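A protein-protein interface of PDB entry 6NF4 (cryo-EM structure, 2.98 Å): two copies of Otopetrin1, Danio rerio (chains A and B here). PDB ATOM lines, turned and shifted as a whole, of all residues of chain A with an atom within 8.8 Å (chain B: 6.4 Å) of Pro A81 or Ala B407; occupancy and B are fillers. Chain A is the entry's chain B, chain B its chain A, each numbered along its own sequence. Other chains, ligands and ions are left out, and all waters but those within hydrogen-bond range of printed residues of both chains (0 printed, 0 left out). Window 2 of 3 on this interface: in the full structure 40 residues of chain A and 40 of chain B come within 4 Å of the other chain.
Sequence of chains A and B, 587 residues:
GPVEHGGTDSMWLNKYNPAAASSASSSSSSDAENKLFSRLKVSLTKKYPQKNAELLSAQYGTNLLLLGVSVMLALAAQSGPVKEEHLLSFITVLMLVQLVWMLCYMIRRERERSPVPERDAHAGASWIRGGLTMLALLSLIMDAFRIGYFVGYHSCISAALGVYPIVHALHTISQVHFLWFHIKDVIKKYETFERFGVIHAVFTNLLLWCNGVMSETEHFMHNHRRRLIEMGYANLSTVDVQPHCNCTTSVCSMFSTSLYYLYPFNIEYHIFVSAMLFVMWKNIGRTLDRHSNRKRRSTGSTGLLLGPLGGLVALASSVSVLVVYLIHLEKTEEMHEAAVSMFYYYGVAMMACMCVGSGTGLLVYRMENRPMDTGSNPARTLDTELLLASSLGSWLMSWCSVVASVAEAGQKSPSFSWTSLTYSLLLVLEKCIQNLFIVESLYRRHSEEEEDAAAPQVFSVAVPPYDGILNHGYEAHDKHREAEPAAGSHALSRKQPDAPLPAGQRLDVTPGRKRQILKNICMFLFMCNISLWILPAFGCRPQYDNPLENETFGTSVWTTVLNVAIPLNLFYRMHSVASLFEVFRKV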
ATOM      1  N   ALA A  74      20.407 -32.077 -18.502  1.00  0.00           N
ATOM      2  CA  ALA A  74      20.461 -30.970 -19.451  1.00  0.00           C
ATOM      3  C   ALA A  74      20.293 -31.460 -20.879  1.00  0.00           C
ATOM      4  O   ALA A  74      19.777 -30.737 -21.736  1.00  0.00           O
ATOM      5  CB  ALA A  74      21.775 -30.211 -19.304  1.00  0.00           C
ATOM      6  N   LEU A  75      20.737 -32.685 -21.155  1.00  0.00           N
ATOM      7  CA  LEU A  75      20.638 -33.244 -22.498  1.00  0.00           C
ATOM      8  C   LEU A  75      19.206 -33.631 -22.842  1.00  0.00           C
ATOM      9  O   LEU A  75      18.754 -33.419 -23.971  1.00  0.00           O
ATOM     10  CB  LEU A  75      21.562 -34.453 -22.617  1.00  0.00           C
ATOM     11  CG  LEU A  75      21.564 -35.184 -23.948  1.00  0.00           C
ATOM     12  CD1 LEU A  75      21.971 -34.239 -25.049  1.00  0.00           C
ATOM     13  CD2 LEU A  75      22.495 -36.365 -23.883  1.00  0.00           C
ATOM     14  N   ALA A  77      16.313 -32.474 -21.783  1.00  0.00           N
ATOM     15  CA  ALA A  77      15.553 -31.276 -22.130  1.00  0.00           C
ATOM     16  C   ALA A  77      16.199 -30.670 -23.369  1.00  0.00           C
ATOM     17  O   ALA A  77      17.119 -29.854 -23.292  1.00  0.00           O
ATOM     18  CB  ALA A  77      15.524 -30.293 -20.970  1.00  0.00           C
ATOM     19  N   GLN A  78      15.709 -31.107 -24.534  1.00  0.00           N
ATOM     20  CA  GLN A  78      16.367 -30.810 -25.806  1.00  0.00           C
ATOM     21  C   GLN A  78      16.337 -29.328 -26.162  1.00  0.00           C
ATOM     22  O   GLN A  78      17.145 -28.875 -26.980  1.00  0.00           O
ATOM     23  CB  GLN A  78      15.734 -31.636 -26.922  1.00  0.00           C
ATOM     24  CG  GLN A  78      15.995 -33.119 -26.781  1.00  0.00           C
ATOM     25  CD  GLN A  78      15.353 -33.926 -27.881  1.00  0.00           C
ATOM     26  OE1 GLN A  78      14.660 -33.382 -28.739  1.00  0.00           O
ATOM     27  NE2 GLN A  78      15.574 -35.234 -27.861  1.00  0.00           N
ATOM     28  N   SER A  79      15.423 -28.557 -25.571  1.00  0.00           N
ATOM     29  CA  SER A  79      15.416 -27.104 -25.732  1.00  0.00           C
ATOM     30  C   SER A  79      16.514 -26.485 -24.863  1.00  0.00           C
ATOM     31  O   SER A  79      16.271 -25.885 -23.816  1.00  0.00           O
ATOM     32  CB  SER A  79      14.048 -26.537 -25.383  1.00  0.00           C
ATOM     33  OG  SER A  79      14.095 -25.124 -25.299  1.00  0.00           O
ATOM     34  N   GLY A  80      17.752 -26.636 -25.327  1.00  0.00           N
ATOM     35  CA  GLY A  80      18.899 -26.137 -24.609  1.00  0.00           C
ATOM     36  C   GLY A  80      20.180 -26.290 -25.402  1.00  0.00           C
ATOM     37  O   GLY A  80      20.206 -26.924 -26.459  1.00  0.00           O
ATOM     38  N   PRO A  81      21.273 -25.702 -24.907  1.00  0.00           N
ATOM     39  CA  PRO A  81      22.531 -25.715 -25.669  1.00  0.00           C
ATOM     40  C   PRO A  81      23.326 -27.004 -25.554  1.00  0.00           C
ATOM     41  O   PRO A  81      24.253 -27.198 -26.349  1.00  0.00           O
ATOM     42  CB  PRO A  81      23.309 -24.544 -25.069  1.00  0.00           C
ATOM     43  CG  PRO A  81      22.821 -24.481 -23.666  1.00  0.00           C
ATOM     44  CD  PRO A  81      21.371 -24.865 -23.700  1.00  0.00           C
ATOM     45  N   VAL A  82      23.017 -27.879 -24.604  1.00  0.00           N
ATOM     46  CA  VAL A  82      23.831 -29.063 -24.346  1.00  0.00           C
ATOM     47  C   VAL A  82      23.420 -30.163 -25.317  1.00  0.00           C
ATOM     48  O   VAL A  82      22.243 -30.526 -25.397  1.00  0.00           O
ATOM     49  CB  VAL A  82      23.691 -29.529 -22.891  1.00  0.00           C
ATOM     50  CG1 VAL A  82      24.504 -30.777 -22.659  1.00  0.00           C
ATOM     51  CG2 VAL A  82      24.131 -28.434 -21.949  1.00  0.00           C
ATOM     52  N   LYS A  83      24.389 -30.684 -26.062  1.00  0.00           N
ATOM     53  CA  LYS A  83      24.166 -31.707 -27.072  1.00  0.00           C
ATOM     54  C   LYS A  83      24.890 -32.990 -26.687  1.00  0.00           C
ATOM     55  O   LYS A  83      25.665 -33.024 -25.730  1.00  0.00           O
ATOM     56  CB  LYS A  83      24.623 -31.203 -28.442  1.00  0.00           C
ATOM     57  CG  LYS A  83      23.941 -29.908 -28.831  1.00  0.00           C
ATOM     58  CD  LYS A  83      24.575 -29.261 -30.040  1.00  0.00           C
ATOM     59  CE  LYS A  83      24.913 -27.810 -29.743  1.00  0.00           C
ATOM     60  NZ  LYS A  83      23.702 -26.946 -29.742  1.00  0.00           N
ATOM     61  N   GLU A  84      24.605 -34.060 -27.443  1.00  0.00           N
ATOM     62  CA  GLU A  84      25.077 -35.397 -27.082  1.00  0.00           C
ATOM     63  C   GLU A  84      26.593 -35.528 -27.172  1.00  0.00           C
ATOM     64  O   GLU A  84      27.190 -36.328 -26.439  1.00  0.00           O
ATOM     65  CB  GLU A  84      24.390 -36.449 -27.955  1.00  0.00           C
ATOM     66  CG  GLU A  84      24.713 -36.357 -29.438  1.00  0.00           C
ATOM     67  CD  GLU A  84      23.958 -37.367 -30.272  1.00  0.00           C
ATOM     68  OE1 GLU A  84      23.136 -38.113 -29.706  1.00  0.00           O
ATOM     69  OE2 GLU A  84      24.195 -37.421 -31.495  1.00  0.00           O
ATOM     70  N   GLU A  85      27.236 -34.745 -28.045  1.00  0.00           N
ATOM     71  CA  GLU A  85      28.689 -34.793 -28.149  1.00  0.00           C
ATOM     72  C   GLU A  85      29.361 -34.239 -26.904  1.00  0.00           C
ATOM     73  O   GLU A  85      30.499 -34.605 -26.605  1.00  0.00           O
ATOM     74  CB  GLU A  85      29.164 -34.044 -29.390  1.00  0.00           C
ATOM     75  CG  GLU A  85      28.590 -32.663 -29.533  1.00  0.00           C
ATOM     76  CD  GLU A  85      27.520 -32.607 -30.594  1.00  0.00           C
ATOM     77  OE1 GLU A  85      26.982 -33.677 -30.947  1.00  0.00           O
ATOM     78  OE2 GLU A  85      27.215 -31.496 -31.074  1.00  0.00           O
ATOM     79  N   HIS A  86      28.667 -33.396 -26.145  1.00  0.00           N
ATOM     80  CA  HIS A  86      29.220 -32.910 -24.888  1.00  0.00           C
ATOM     81  C   HIS A  86      29.231 -34.005 -23.829  1.00  0.00           C
ATOM     82  O   HIS A  86      30.208 -34.138 -23.080  1.00  0.00           O
ATOM     83  CB  HIS A  86      28.424 -31.699 -24.420  1.00  0.00           C
ATOM     84  CG  HIS A  86      28.397 -30.589 -25.420  1.00  0.00           C
ATOM     85  ND1 HIS A  86      27.336 -29.720 -25.541  1.00  0.00           N
ATOM     86  CD2 HIS A  86      29.300 -30.213 -26.354  1.00  0.00           C
ATOM     87  CE1 HIS A  86      27.590 -28.854 -26.505  1.00  0.00           C
ATOM     88  NE2 HIS A  86      28.776 -29.131 -27.014  1.00  0.00           N
ATOM     89  N   VAL B 402      26.020 -25.469 -12.135  1.00  0.00           N
ATOM     90  CA  VAL B 402      27.330 -25.360 -12.778  1.00  0.00           C
ATOM     91  C   VAL B 402      27.232 -25.700 -14.260  1.00  0.00           C
ATOM     92  O   VAL B 402      27.796 -25.000 -15.107  1.00  0.00           O
ATOM     93  CB  VAL B 402      28.354 -26.251 -12.052  1.00  0.00           C
ATOM     94  CG1 VAL B 402      29.609 -26.429 -12.868  1.00  0.00           C
ATOM     95  CG2 VAL B 402      28.723 -25.640 -10.730  1.00  0.00           C
ATOM     96  N   VAL B 403      26.490 -26.761 -14.593  1.00  0.00           N
ATOM     97  CA  VAL B 403      26.317 -27.163 -15.988  1.00  0.00           C
ATOM     98  C   VAL B 403      25.571 -26.092 -16.774  1.00  0.00           C
ATOM     99  O   VAL B 403      25.964 -25.752 -17.897  1.00  0.00           O
ATOM    100  CB  VAL B 403      25.621 -28.535 -16.061  1.00  0.00           C
ATOM    101  CG1 VAL B 403      25.125 -28.833 -17.451  1.00  0.00           C
ATOM    102  CG2 VAL B 403      26.587 -29.616 -15.649  1.00  0.00           C
ATOM    103  N   ALA B 404      24.533 -25.494 -16.176  1.00  0.00           N
ATOM    104  CA  ALA B 404      23.792 -24.436 -16.864  1.00  0.00           C
ATOM    105  C   ALA B 404      24.643 -23.188 -17.085  1.00  0.00           C
ATOM    106  O   ALA B 404      24.615 -22.598 -18.173  1.00  0.00           O
ATOM    107  CB  ALA B 404      22.535 -24.083 -16.081  1.00  0.00           C
ATOM    108  N   SER B 405      25.430 -22.789 -16.080  1.00  0.00           N
ATOM    109  CA  SER B 405      26.257 -21.593 -16.225  1.00  0.00           C
ATOM    110  C   SER B 405      27.402 -21.804 -17.210  1.00  0.00           C
ATOM    111  O   SER B 405      27.728 -20.898 -17.978  1.00  0.00           O
ATOM    112  CB  SER B 405      26.789 -21.151 -14.867  1.00  0.00           C
ATOM    113  OG  SER B 405      27.319 -22.245 -14.149  1.00  0.00           O
ATOM    114  N   VAL B 406      28.019 -22.987 -17.210  1.00  0.00           N
ATOM    115  CA  VAL B 406      29.086 -23.278 -18.169  1.00  0.00           C
ATOM    116  C   VAL B 406      28.532 -23.367 -19.589  1.00  0.00           C
ATOM    117  O   VAL B 406      29.151 -22.872 -20.542  1.00  0.00           O
ATOM    118  CB  VAL B 406      29.831 -24.559 -17.746  1.00  0.00           C
ATOM    119  CG1 VAL B 406      30.714 -25.093 -18.851  1.00  0.00           C
ATOM    120  CG2 VAL B 406      30.684 -24.273 -16.532  1.00  0.00           C
ATOM    121  N   ALA B 407      27.344 -23.959 -19.752  1.00  0.00           N
ATOM    122  CA  ALA B 407      26.707 -24.003 -21.065  1.00  0.00           C
ATOM    123  C   ALA B 407      26.333 -22.610 -21.559  1.00  0.00           C
ATOM    124  O   ALA B 407      26.353 -22.353 -22.767  1.00  0.00           O
ATOM    125  CB  ALA B 407      25.476 -24.904 -21.023  1.00  0.00           C
ATOM    126  N   GLU B 408      25.986 -21.696 -20.649  1.00  0.00           N
ATOM    127  CA  GLU B 408      25.715 -20.326 -21.080  1.00  0.00           C
ATOM    128  C   GLU B 408      27.012 -19.580 -21.390  1.00  0.00           C
ATOM    129  O   GLU B 408      27.048 -18.733 -22.288  1.00  0.00           O
ATOM    130  CB  GLU B 408      24.933 -19.568 -20.014  1.00  0.00           C
ATOM    131  CG  GLU B 408      24.243 -18.335 -20.551  1.00  0.00           C
ATOM    132  CD  GLU B 408      23.793 -17.373 -19.479  1.00  0.00           C
ATOM    133  OE1 GLU B 408      24.176 -17.563 -18.307  1.00  0.00           O
ATOM    134  OE2 GLU B 408      23.048 -16.422 -19.805  1.00  0.00           O
ATOM    135  N   ALA B 409      28.075 -19.864 -20.630  1.00  0.00           N
ATOM    136  CA  ALA B 409      29.373 -19.227 -20.855  1.00  0.00           C
ATOM    137  C   ALA B 409      29.984 -19.654 -22.179  1.00  0.00           C
ATOM    138  O   ALA B 409      30.751 -18.901 -22.789  1.00  0.00           O
ATOM    139  CB  ALA B 409      30.329 -19.562 -19.712  1.00  0.00           C
ATOM    140  N   GLY B 410      29.669 -20.869 -22.629  1.00  0.00           N
ATOM    141  CA  GLY B 410      30.134 -21.356 -23.920  1.00  0.00           C
ATOM    142  C   GLY B 410      29.600 -20.601 -25.125  1.00  0.00           C
ATOM    143  O   GLY B 410      30.074 -20.829 -26.242  1.00  0.00           O
ATOM    144  N   GLN B 411      28.610 -19.727 -24.933  1.00  0.00           N
ATOM    145  CA  GLN B 411      28.100 -18.858 -25.983  1.00  0.00           C
ATOM    146  C   GLN B 411      28.731 -17.469 -25.952  1.00  0.00           C
ATOM    147  O   GLN B 411      28.430 -16.657 -26.833  1.00  0.00           O
ATOM    148  CB  GLN B 411      26.580 -18.722 -25.853  1.00  0.00           C
ATOM    149  CG  GLN B 411      25.831 -20.041 -25.855  1.00  0.00           C
ATOM    150  CD  GLN B 411      26.009 -20.816 -27.139  1.00  0.00           C
ATOM    151  OE1 GLN B 411      26.720 -21.819 -27.176  1.00  0.00           O
ATOM    152  NE2 GLN B 411      25.351 -20.362 -28.199  1.00  0.00           N
ATOM    153  N   SER B 413      27.957 -15.263 -23.760  1.00  0.00           N
ATOM    154  CA  SER B 413      26.724 -14.533 -23.557  1.00  0.00           C
ATOM    155  C   SER B 413      26.885 -13.448 -22.497  1.00  0.00           C
ATOM    156  O   SER B 413      27.825 -13.480 -21.699  1.00  0.00           O
ATOM    157  CB  SER B 413      25.647 -15.517 -23.130  1.00  0.00           C
ATOM    158  OG  SER B 413      26.198 -16.408 -22.183  1.00  0.00           O
ATOM    159  N   GLU B 551      14.818 -22.970 -18.677  1.00  0.00           N
ATOM    160  CA  GLU B 551      15.174 -22.865 -20.103  1.00  0.00           C
ATOM    161  C   GLU B 551      16.429 -23.680 -20.455  1.00  0.00           C
ATOM    162  O   GLU B 551      16.730 -23.883 -21.637  1.00  0.00           O
ATOM    163  CB  GLU B 551      15.261 -21.378 -20.539  1.00  0.00           C
ATOM    164  CG  GLU B 551      15.597 -20.989 -21.967  1.00  0.00           C
ATOM    165  CD  GLU B 551      17.090 -20.802 -22.144  1.00  0.00           C
ATOM    166  OE1 GLU B 551      17.762 -20.449 -21.152  1.00  0.00           O
ATOM    167  OE2 GLU B 551      17.594 -20.999 -23.264  1.00  0.00           O
ATOM    168  N   THR B 552      17.089 -24.286 -19.473  1.00  0.00           N
ATOM    169  CA  THR B 552      18.145 -25.261 -19.704  1.00  0.00           C
ATOM    170  C   THR B 552      17.683 -26.666 -19.369  1.00  0.00           C
ATOM    171  O   THR B 552      17.904 -27.594 -20.156  1.00  0.00           O
ATOM    172  CB  THR B 552      19.385 -24.910 -18.869  1.00  0.00           C
ATOM    173  OG1 THR B 552      19.845 -23.606 -19.224  1.00  0.00           O
ATOM    174  CG2 THR B 552      20.498 -25.891 -19.120  1.00  0.00           C
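The backbone carbonyl oxygen (O) of Glu B551 lies close to the backbone carbonyl oxygen (O) of Ser A79.
NZ of Lys A83 lies within hydrogen-bond range of O of Pro A81, at 3.4 Å.
Among the printed residues, pairs that only touch across the chains: Ala A74 with Thr B552, Ala A77 with Thr B552, Pro A81 with Ala B407 and Val A82 with Ala B407.
Printed residues of chain B within 4 Å of Ala A74: Thr B552 (3.99 Å).
Of chain B, only Ala B407 comes within 4 Å of Pro A81.
Of the printed residues of chain B, Val A82 touches Ala B407.
No residue of chain A comes within 4 Å of Val B406.
Of chain A, only Pro A81 (3.8 Å) and Val A82 (3.9 Å) come within 4 Å of Ala B407.
Of the printed residues of chain A, Glu B551 touches Ser A79 (3.0 Å).
Of the printed residues of chain A, Thr B552 touches Ala A74 and Ala A77.
The nearest residue of chain A that does not touch Ala B407 is Ala A74 (6.7 Å).
The nearest printed residue of chain A that does not touch Glu B551 is Gly A80 (4.3 Å).
Printed residues of chain A that touch a printed residue of chain B: Ala A74, Ala A77, Ser A79, Pro A81 and Val A82.
Hydrophobic or aromatic side chains of chain A within 4 Å of the printed part of chain B: Ala A77, Pro A81 and Val A82.
Printed residues of chain B that touch a printed residue of chain A: Ala B407, Glu B551 and Thr B552.
Among the printed residues, 5 pairs touch across the chains.
No position is printed for both chains.
Of the 5 pairs that touch across the chains among the printed residues, none has its exchanged pair printed and touching as well.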
